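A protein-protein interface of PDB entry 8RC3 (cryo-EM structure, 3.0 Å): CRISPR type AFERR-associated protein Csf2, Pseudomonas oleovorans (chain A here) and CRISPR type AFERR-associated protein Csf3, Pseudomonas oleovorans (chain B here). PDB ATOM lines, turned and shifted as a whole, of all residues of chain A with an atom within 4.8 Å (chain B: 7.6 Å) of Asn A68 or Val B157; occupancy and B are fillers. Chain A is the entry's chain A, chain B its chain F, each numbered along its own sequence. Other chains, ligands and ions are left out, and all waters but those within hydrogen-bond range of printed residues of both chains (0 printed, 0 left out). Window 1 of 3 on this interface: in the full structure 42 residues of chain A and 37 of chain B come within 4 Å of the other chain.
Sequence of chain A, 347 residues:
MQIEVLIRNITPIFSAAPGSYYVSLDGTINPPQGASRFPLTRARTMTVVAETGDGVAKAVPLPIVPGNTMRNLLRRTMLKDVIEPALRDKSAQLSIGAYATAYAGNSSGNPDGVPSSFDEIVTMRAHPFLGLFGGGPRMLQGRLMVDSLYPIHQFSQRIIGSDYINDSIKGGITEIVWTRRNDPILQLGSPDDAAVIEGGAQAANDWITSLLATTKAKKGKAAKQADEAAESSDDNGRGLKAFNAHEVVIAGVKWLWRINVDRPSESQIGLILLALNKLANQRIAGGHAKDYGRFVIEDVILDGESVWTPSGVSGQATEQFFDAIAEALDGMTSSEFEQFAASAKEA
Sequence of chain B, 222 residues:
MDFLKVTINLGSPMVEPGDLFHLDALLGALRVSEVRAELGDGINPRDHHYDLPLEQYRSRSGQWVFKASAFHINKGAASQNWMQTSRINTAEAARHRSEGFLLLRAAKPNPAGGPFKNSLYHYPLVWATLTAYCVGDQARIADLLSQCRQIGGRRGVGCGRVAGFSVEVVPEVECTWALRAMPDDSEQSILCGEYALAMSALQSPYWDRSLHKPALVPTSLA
The side-chain amide nitrogen (ND2) of Asn A68 lies within hydrogen-bond range of the side-chain hydroxyl (OH) of Tyr B121.
The guanidinium group of Arg A71 lies within hydrogen-bond range of the backbone carbonyl oxygen of Gly B156 (3.2 Å).
The backbone NH (N) of Val A146 sits at hydrogen-bond distance from the backbone carbonyl oxygen (O) of Gly B156 (3.0 Å).
The backbone carbonyl oxygen (O) of Val A146 lies within hydrogen-bond range of the backbone NH (N) of Gly B158.
O of Val A146 sits close to O of Val B157.
The side-chain hydroxyl (OG) of Ser A148 is in hydrogen-bond range of the backbone NH (N) of Gly A67 (3.1 Å).
NE2 of Gln B84 lies within hydrogen-bond range of OH of Tyr B121 (2.6 Å).
OH of Tyr B123 sits at hydrogen-bond distance from OE1 of Gln B84, at 2.4 Å.
Among the printed residues, pairs that only touch across the chains: Gly A67 with Val B157, Asn A68 with Gln B84, Asn A68 with Thr B85, Asn A68 with Val B157 and Asp A147 with Gly B158.
Gly A67 touches just one residue of chain B: Val B157.
Of chain B, only Gln B84, Thr B85, Tyr B121 and Val B157 come within 4 Å of Asn A68.
Printed residues of chain B within 4 Å of Asp A147: Gly B158 (3.1 Å).
Leu B125 touches none of the printed residues of chain A.
Of the printed residues of chain A, Gly B156 touches Arg A71 (3.2 Å) and Val A146 (3.0 Å).
Of the printed residues of chain A, Val B157 touches Gly A67 (3.8 Å), Asn A68 (3.8 Å) and Val A146 (2.9 Å).
The nearest printed residue of chain A that does not touch Val B157 is Arg A71 (4.001 Å).
Of the 18 printed residues of chain B, 6 touch a printed residue of chain A.
Hydrophobic or aromatic side chains of chain A within 4 Å of the printed part of chain B: Val A146.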
ATOM      1  N   PRO A  66      25.151 -11.341  14.945  1.00  0.00           N
ATOM      2  CA  PRO A  66      25.790 -12.328  15.821  1.00  0.00           C
ATOM      3  C   PRO A  66      26.816 -11.701  16.750  1.00  0.00           C
ATOM      4  O   PRO A  66      27.432 -10.681  16.439  1.00  0.00           O
ATOM      5  CB  PRO A  66      26.451 -13.295  14.835  1.00  0.00           C
ATOM      6  CG  PRO A  66      25.666 -13.154  13.597  1.00  0.00           C
ATOM      7  CD  PRO A  66      25.250 -11.721  13.530  1.00  0.00           C
ATOM      8  N   GLY A  67      26.980 -12.326  17.917  1.00  0.00           N
ATOM      9  CA  GLY A  67      27.924 -11.822  18.895  1.00  0.00           C
ATOM     10  C   GLY A  67      29.359 -11.863  18.419  1.00  0.00           C
ATOM     11  O   GLY A  67      30.165 -11.013  18.799  1.00  0.00           O
ATOM     12  N   ASN A  68      29.706 -12.856  17.599  1.00  0.00           N
ATOM     13  CA  ASN A  68      31.055 -12.914  17.047  1.00  0.00           C
ATOM     14  C   ASN A  68      31.317 -11.739  16.117  1.00  0.00           C
ATOM     15  O   ASN A  68      32.423 -11.184  16.099  1.00  0.00           O
ATOM     16  CB  ASN A  68      31.266 -14.234  16.313  1.00  0.00           C
ATOM     17  CG  ASN A  68      32.722 -14.603  16.203  1.00  0.00           C
ATOM     18  OD1 ASN A  68      33.571 -14.016  16.869  1.00  0.00           O
ATOM     19  ND2 ASN A  68      33.021 -15.584  15.364  1.00  0.00           N
ATOM     20  N   THR A  69      30.307 -11.345  15.342  1.00  0.00           N
ATOM     21  CA  THR A  69      30.459 -10.203  14.450  1.00  0.00           C
ATOM     22  C   THR A  69      30.783  -8.942  15.232  1.00  0.00           C
ATOM     23  O   THR A  69      31.666  -8.172  14.843  1.00  0.00           O
ATOM     24  CB  THR A  69      29.191 -10.009  13.622  1.00  0.00           C
ATOM     25  OG1 THR A  69      28.967 -11.166  12.812  1.00  0.00           O
ATOM     26  CG2 THR A  69      29.322  -8.799  12.729  1.00  0.00           C
ATOM     27  N   MET A  70      30.106  -8.725  16.357  1.00  0.00           N
ATOM     28  CA  MET A  70      30.349  -7.508  17.118  1.00  0.00           C
ATOM     29  C   MET A  70      31.608  -7.598  17.968  1.00  0.00           C
ATOM     30  O   MET A  70      32.252  -6.576  18.221  1.00  0.00           O
ATOM     31  CB  MET A  70      29.139  -7.183  17.982  1.00  0.00           C
ATOM     32  CG  MET A  70      27.845  -7.242  17.211  1.00  0.00           C
ATOM     33  SD  MET A  70      26.707  -5.987  17.780  1.00  0.00           S
ATOM     34  CE  MET A  70      27.574  -4.525  17.228  1.00  0.00           C
ATOM     35  N   ARG A  71      31.985  -8.803  18.396  1.00  0.00           N
ATOM     36  CA  ARG A  71      33.295  -9.000  19.005  1.00  0.00           C
ATOM     37  C   ARG A  71      34.398  -8.574  18.047  1.00  0.00           C
ATOM     38  O   ARG A  71      35.295  -7.799  18.406  1.00  0.00           O
ATOM     39  CB  ARG A  71      33.456 -10.467  19.400  1.00  0.00           C
ATOM     40  CG  ARG A  71      34.759 -10.803  20.078  1.00  0.00           C
ATOM     41  CD  ARG A  71      34.583 -10.833  21.575  1.00  0.00           C
ATOM     42  NE  ARG A  71      35.770 -11.325  22.260  1.00  0.00           N
ATOM     43  CZ  ARG A  71      35.893 -12.544  22.761  1.00  0.00           C
ATOM     44  NH1 ARG A  71      34.918 -13.431  22.661  1.00  0.00           N
ATOM     45  NH2 ARG A  71      37.020 -12.880  23.377  1.00  0.00           N
ATOM     46  N   ASN A  72      34.327  -9.053  16.804  1.00  0.00           N
ATOM     47  CA  ASN A  72      35.312  -8.656  15.807  1.00  0.00           C
ATOM     48  C   ASN A  72      35.197  -7.180  15.453  1.00  0.00           C
ATOM     49  O   ASN A  72      36.208  -6.548  15.141  1.00  0.00           O
ATOM     50  CB  ASN A  72      35.174  -9.507  14.552  1.00  0.00           C
ATOM     51  CG  ASN A  72      36.055  -9.020  13.430  1.00  0.00           C
ATOM     52  OD1 ASN A  72      35.575  -8.461  12.447  1.00  0.00           O
ATOM     53  ND2 ASN A  72      37.359  -9.210  13.578  1.00  0.00           N
ATOM     54  N   VAL A 146      31.183 -10.250  24.895  1.00  0.00           N
ATOM     55  CA  VAL A 146      30.206  -9.404  24.223  1.00  0.00           C
ATOM     56  C   VAL A 146      28.997 -10.246  23.850  1.00  0.00           C
ATOM     57  O   VAL A 146      29.096 -11.459  23.655  1.00  0.00           O
ATOM     58  CB  VAL A 146      30.813  -8.728  22.978  1.00  0.00           C
ATOM     59  CG1 VAL A 146      32.056  -7.950  23.352  1.00  0.00           C
ATOM     60  CG2 VAL A 146      31.121  -9.759  21.931  1.00  0.00           C
ATOM     61  N   ASP A 147      27.841  -9.602  23.765  1.00  0.00           N
ATOM     62  CA  ASP A 147      26.609 -10.264  23.365  1.00  0.00           C
ATOM     63  C   ASP A 147      26.254  -9.897  21.929  1.00  0.00           C
ATOM     64  O   ASP A 147      26.891  -9.054  21.296  1.00  0.00           O
ATOM     65  CB  ASP A 147      25.464  -9.892  24.308  1.00  0.00           C
ATOM     66  CG  ASP A 147      25.637 -10.472  25.692  1.00  0.00           C
ATOM     67  OD1 ASP A 147      26.262 -11.544  25.818  1.00  0.00           O
ATOM     68  OD2 ASP A 147      25.145  -9.859  26.661  1.00  0.00           O
ATOM     69  N   SER A 148      25.216 -10.549  21.418  1.00  0.00           N
ATOM     70  CA  SER A 148      24.705 -10.216  20.101  1.00  0.00           C
ATOM     71  C   SER A 148      23.980  -8.874  20.146  1.00  0.00           C
ATOM     72  O   SER A 148      23.741  -8.299  21.210  1.00  0.00           O
ATOM     73  CB  SER A 148      23.767 -11.311  19.602  1.00  0.00           C
ATOM     74  OG  SER A 148      24.383 -12.583  19.674  1.00  0.00           O
ATOM     75  N   VAL B  15      25.040 -22.963  24.123  1.00  0.00           N
ATOM     76  CA  VAL B  15      25.599 -23.924  23.183  1.00  0.00           C
ATOM     77  C   VAL B  15      25.294 -25.317  23.707  1.00  0.00           C
ATOM     78  O   VAL B  15      25.669 -25.662  24.832  1.00  0.00           O
ATOM     79  CB  VAL B  15      27.107 -23.714  23.003  1.00  0.00           C
ATOM     80  CG1 VAL B  15      27.669 -24.734  22.037  1.00  0.00           C
ATOM     81  CG2 VAL B  15      27.373 -22.313  22.515  1.00  0.00           C
ATOM     82  N   TRP B  82      24.216 -22.785  14.706  1.00  0.00           N
ATOM     83  CA  TRP B  82      24.764 -21.439  14.626  1.00  0.00           C
ATOM     84  C   TRP B  82      26.083 -21.464  13.870  1.00  0.00           C
ATOM     85  O   TRP B  82      27.000 -22.203  14.235  1.00  0.00           O
ATOM     86  CB  TRP B  82      24.967 -20.855  16.020  1.00  0.00           C
ATOM     87  CG  TRP B  82      24.991 -19.367  16.054  1.00  0.00           C
ATOM     88  CD1 TRP B  82      26.047 -18.575  16.375  1.00  0.00           C
ATOM     89  CD2 TRP B  82      23.902 -18.485  15.767  1.00  0.00           C
ATOM     90  NE1 TRP B  82      25.688 -17.253  16.306  1.00  0.00           N
ATOM     91  CE2 TRP B  82      24.374 -17.173  15.934  1.00  0.00           C
ATOM     92  CE3 TRP B  82      22.574 -18.679  15.384  1.00  0.00           C
ATOM     93  CZ2 TRP B  82      23.568 -16.061  15.730  1.00  0.00           C
ATOM     94  CZ3 TRP B  82      21.777 -17.575  15.184  1.00  0.00           C
ATOM     95  CH2 TRP B  82      22.275 -16.283  15.357  1.00  0.00           C
ATOM     96  N   MET B  83      26.175 -20.647  12.829  1.00  0.00           N
ATOM     97  CA  MET B  83      27.360 -20.574  11.992  1.00  0.00           C
ATOM     98  C   MET B  83      28.216 -19.385  12.394  1.00  0.00           C
ATOM     99  O   MET B  83      27.705 -18.287  12.625  1.00  0.00           O
ATOM    100  CB  MET B  83      26.981 -20.457  10.516  1.00  0.00           C
ATOM    101  CG  MET B  83      28.144 -20.644   9.566  1.00  0.00           C
ATOM    102  SD  MET B  83      27.999 -19.588   8.119  1.00  0.00           S
ATOM    103  CE  MET B  83      27.913 -17.977   8.890  1.00  0.00           C
ATOM    104  N   GLN B  84      29.519 -19.617  12.489  1.00  0.00           N
ATOM    105  CA  GLN B  84      30.484 -18.556  12.715  1.00  0.00           C
ATOM    106  C   GLN B  84      31.674 -18.789  11.803  1.00  0.00           C
ATOM    107  O   GLN B  84      31.960 -19.922  11.411  1.00  0.00           O
ATOM    108  CB  GLN B  84      30.941 -18.500  14.172  1.00  0.00           C
ATOM    109  CG  GLN B  84      30.021 -17.730  15.087  1.00  0.00           C
ATOM    110  CD  GLN B  84      30.432 -17.848  16.535  1.00  0.00           C
ATOM    111  OE1 GLN B  84      29.723 -17.399  17.431  1.00  0.00           O
ATOM    112  NE2 GLN B  84      31.583 -18.457  16.772  1.00  0.00           N
ATOM    113  N   THR B  85      32.358 -17.706  11.456  1.00  0.00           N
ATOM    114  CA  THR B  85      33.504 -17.768  10.567  1.00  0.00           C
ATOM    115  C   THR B  85      34.698 -17.116  11.248  1.00  0.00           C
ATOM    116  O   THR B  85      34.617 -16.656  12.389  1.00  0.00           O
ATOM    117  CB  THR B  85      33.211 -17.088   9.225  1.00  0.00           C
ATOM    118  OG1 THR B  85      33.110 -15.676   9.415  1.00  0.00           O
ATOM    119  CG2 THR B  85      31.907 -17.591   8.655  1.00  0.00           C
ATOM    120  N   SER B  86      35.822 -17.096  10.541  1.00  0.00           N
ATOM    121  CA  SER B  86      37.012 -16.400  11.002  1.00  0.00           C
ATOM    122  C   SER B  86      37.822 -16.009   9.782  1.00  0.00           C
ATOM    123  O   SER B  86      38.116 -16.856   8.935  1.00  0.00           O
ATOM    124  CB  SER B  86      37.852 -17.272  11.938  1.00  0.00           C
ATOM    125  OG  SER B  86      38.534 -18.279  11.217  1.00  0.00           O
ATOM    126  N   TYR B 121      32.766 -22.834  10.726  1.00  0.00           N
ATOM    127  CA  TYR B 121      32.437 -23.811  11.749  1.00  0.00           C
ATOM    128  C   TYR B 121      31.048 -23.519  12.295  1.00  0.00           C
ATOM    129  O   TYR B 121      30.563 -22.388  12.241  1.00  0.00           O
ATOM    130  CB  TYR B 121      33.467 -23.816  12.884  1.00  0.00           C
ATOM    131  CG  TYR B 121      33.586 -22.505  13.615  1.00  0.00           C
ATOM    132  CD1 TYR B 121      34.374 -21.482  13.119  1.00  0.00           C
ATOM    133  CD2 TYR B 121      32.915 -22.292  14.806  1.00  0.00           C
ATOM    134  CE1 TYR B 121      34.484 -20.287  13.783  1.00  0.00           C
ATOM    135  CE2 TYR B 121      33.020 -21.099  15.474  1.00  0.00           C
ATOM    136  CZ  TYR B 121      33.810 -20.101  14.962  1.00  0.00           C
ATOM    137  OH  TYR B 121      33.916 -18.907  15.630  1.00  0.00           O
ATOM    138  N   TYR B 123      28.100 -24.587  15.563  1.00  0.00           N
ATOM    139  CA  TYR B 123      27.747 -25.183  16.842  1.00  0.00           C
ATOM    140  C   TYR B 123      26.267 -24.944  17.097  1.00  0.00           C
ATOM    141  O   TYR B 123      25.710 -23.949  16.620  1.00  0.00           O
ATOM    142  CB  TYR B 123      28.581 -24.605  17.995  1.00  0.00           C
ATOM    143  CG  TYR B 123      28.496 -23.108  18.144  1.00  0.00           C
ATOM    144  CD1 TYR B 123      27.498 -22.520  18.904  1.00  0.00           C
ATOM    145  CD2 TYR B 123      29.421 -22.281  17.536  1.00  0.00           C
ATOM    146  CE1 TYR B 123      27.420 -21.157  19.044  1.00  0.00           C
ATOM    147  CE2 TYR B 123      29.349 -20.915  17.672  1.00  0.00           C
ATOM    148  CZ  TYR B 123      28.347 -20.361  18.427  1.00  0.00           C
ATOM    149  OH  TYR B 123      28.272 -18.998  18.567  1.00  0.00           O
ATOM    150  N   LEU B 125      22.726 -24.063  19.088  1.00  0.00           N
ATOM    151  CA  LEU B 125      22.187 -23.220  20.145  1.00  0.00           C
ATOM    152  C   LEU B 125      20.833 -23.761  20.579  1.00  0.00           C
ATOM    153  O   LEU B 125      20.004 -24.125  19.739  1.00  0.00           O
ATOM    154  CB  LEU B 125      22.038 -21.770  19.679  1.00  0.00           C
ATOM    155  CG  LEU B 125      23.270 -20.870  19.740  1.00  0.00           C
ATOM    156  CD1 LEU B 125      22.858 -19.420  19.635  1.00  0.00           C
ATOM    157  CD2 LEU B 125      24.058 -21.112  21.007  1.00  0.00           C
ATOM    158  N   GLN B 150      26.855 -17.057  32.768  1.00  0.00           N
ATOM    159  CA  GLN B 150      26.561 -17.773  31.540  1.00  0.00           C
ATOM    160  C   GLN B 150      26.796 -19.265  31.710  1.00  0.00           C
ATOM    161  O   GLN B 150      27.617 -19.696  32.522  1.00  0.00           O
ATOM    162  CB  GLN B 150      27.392 -17.229  30.384  1.00  0.00           C
ATOM    163  CG  GLN B 150      26.983 -15.827  29.992  1.00  0.00           C
ATOM    164  CD  GLN B 150      27.959 -15.168  29.059  1.00  0.00           C
ATOM    165  OE1 GLN B 150      28.922 -15.784  28.617  1.00  0.00           O
ATOM    166  NE2 GLN B 150      27.715 -13.904  28.750  1.00  0.00           N
ATOM    167  N   GLY B 153      29.401 -23.405  26.534  1.00  0.00           N
ATOM    168  CA  GLY B 153      30.546 -22.905  25.811  1.00  0.00           C
ATOM    169  C   GLY B 153      30.226 -21.640  25.045  1.00  0.00           C
ATOM    170  O   GLY B 153      29.121 -21.107  25.097  1.00  0.00           O
ATOM    171  N   ARG B 154      31.235 -21.161  24.322  1.00  0.00           N
ATOM    172  CA  ARG B 154      31.120 -19.961  23.499  1.00  0.00           C
ATOM    173  C   ARG B 154      30.614 -18.781  24.322  1.00  0.00           C
ATOM    174  O   ARG B 154      29.781 -17.992  23.875  1.00  0.00           O
ATOM    175  CB  ARG B 154      30.219 -20.214  22.293  1.00  0.00           C
ATOM    176  CG  ARG B 154      30.857 -21.084  21.231  1.00  0.00           C
ATOM    177  CD  ARG B 154      32.236 -20.571  20.872  1.00  0.00           C
ATOM    178  NE  ARG B 154      32.707 -21.092  19.597  1.00  0.00           N
ATOM    179  CZ  ARG B 154      33.090 -22.345  19.399  1.00  0.00           C
ATOM    180  NH1 ARG B 154      33.063 -23.239  20.370  1.00  0.00           N
ATOM    181  NH2 ARG B 154      33.514 -22.710  18.194  1.00  0.00           N
ATOM    182  N   ARG B 155      31.122 -18.669  25.549  1.00  0.00           N
ATOM    183  CA  ARG B 155      30.697 -17.590  26.431  1.00  0.00           C
ATOM    184  C   ARG B 155      31.230 -16.241  25.971  1.00  0.00           C
ATOM    185  O   ARG B 155      30.639 -15.205  26.288  1.00  0.00           O
ATOM    186  CB  ARG B 155      31.150 -17.873  27.860  1.00  0.00           C
ATOM    187  CG  ARG B 155      30.476 -19.061  28.496  1.00  0.00           C
ATOM    188  CD  ARG B 155      30.797 -19.143  29.968  1.00  0.00           C
ATOM    189  NE  ARG B 155      32.228 -19.232  30.219  1.00  0.00           N
ATOM    190  CZ  ARG B 155      32.962 -20.315  30.007  1.00  0.00           C
ATOM    191  NH1 ARG B 155      32.433 -21.425  29.525  1.00  0.00           N
ATOM    192  NH2 ARG B 155      34.263 -20.281  30.286  1.00  0.00           N
ATOM    193  N   GLY B 156      32.340 -16.231  25.236  1.00  0.00           N
ATOM    194  CA  GLY B 156      32.909 -14.972  24.790  1.00  0.00           C
ATOM    195  C   GLY B 156      31.999 -14.204  23.858  1.00  0.00           C
ATOM    196  O   GLY B 156      31.996 -12.971  23.863  1.00  0.00           O
ATOM    197  N   VAL B 157      31.221 -14.911  23.049  1.00  0.00           N
ATOM    198  CA  VAL B 157      30.291 -14.286  22.125  1.00  0.00           C
ATOM    199  C   VAL B 157      28.889 -14.182  22.728  1.00  0.00           C
ATOM    200  O   VAL B 157      27.919 -13.969  22.008  1.00  0.00           O
ATOM    201  CB  VAL B 157      30.265 -15.016  20.778  1.00  0.00           C
ATOM    202  CG1 VAL B 157      31.637 -14.980  20.145  1.00  0.00           C
ATOM    203  CG2 VAL B 157      29.806 -16.440  20.961  1.00  0.00           C
ATOM    204  N   GLY B 158      28.774 -14.323  24.044  1.00  0.00           N
ATOM    205  CA  GLY B 158      27.514 -14.127  24.729  1.00  0.00           C
ATOM    206  C   GLY B 158      26.483 -15.194  24.450  1.00  0.00           C
ATOM    207  O   GLY B 158      25.408 -14.905  23.919  1.00  0.00           O
ATOM    208  N   CYS B 159      26.797 -16.436  24.804  1.00  0.00           N
ATOM    209  CA  CYS B 159      25.898 -17.563  24.600  1.00  0.00           C
ATOM    210  C   CYS B 159      25.595 -18.205  25.944  1.00  0.00           C
ATOM    211  O   CYS B 159      26.508 -18.663  26.635  1.00  0.00           O
ATOM    212  CB  CYS B 159      26.510 -18.588  23.642  1.00  0.00           C
ATOM    213  SG  CYS B 159      26.562 -18.061  21.919  1.00  0.00           S
ATOM    214  N   GLY B 160      24.316 -18.238  26.308  1.00  0.00           N
ATOM    215  CA  GLY B 160      23.880 -18.966  27.481  1.00  0.00           C
ATOM    216  C   GLY B 160      23.725 -18.134  28.735  1.00  0.00           C
ATOM    217  O   GLY B 160      24.014 -18.615  29.832  1.00  0.00           O
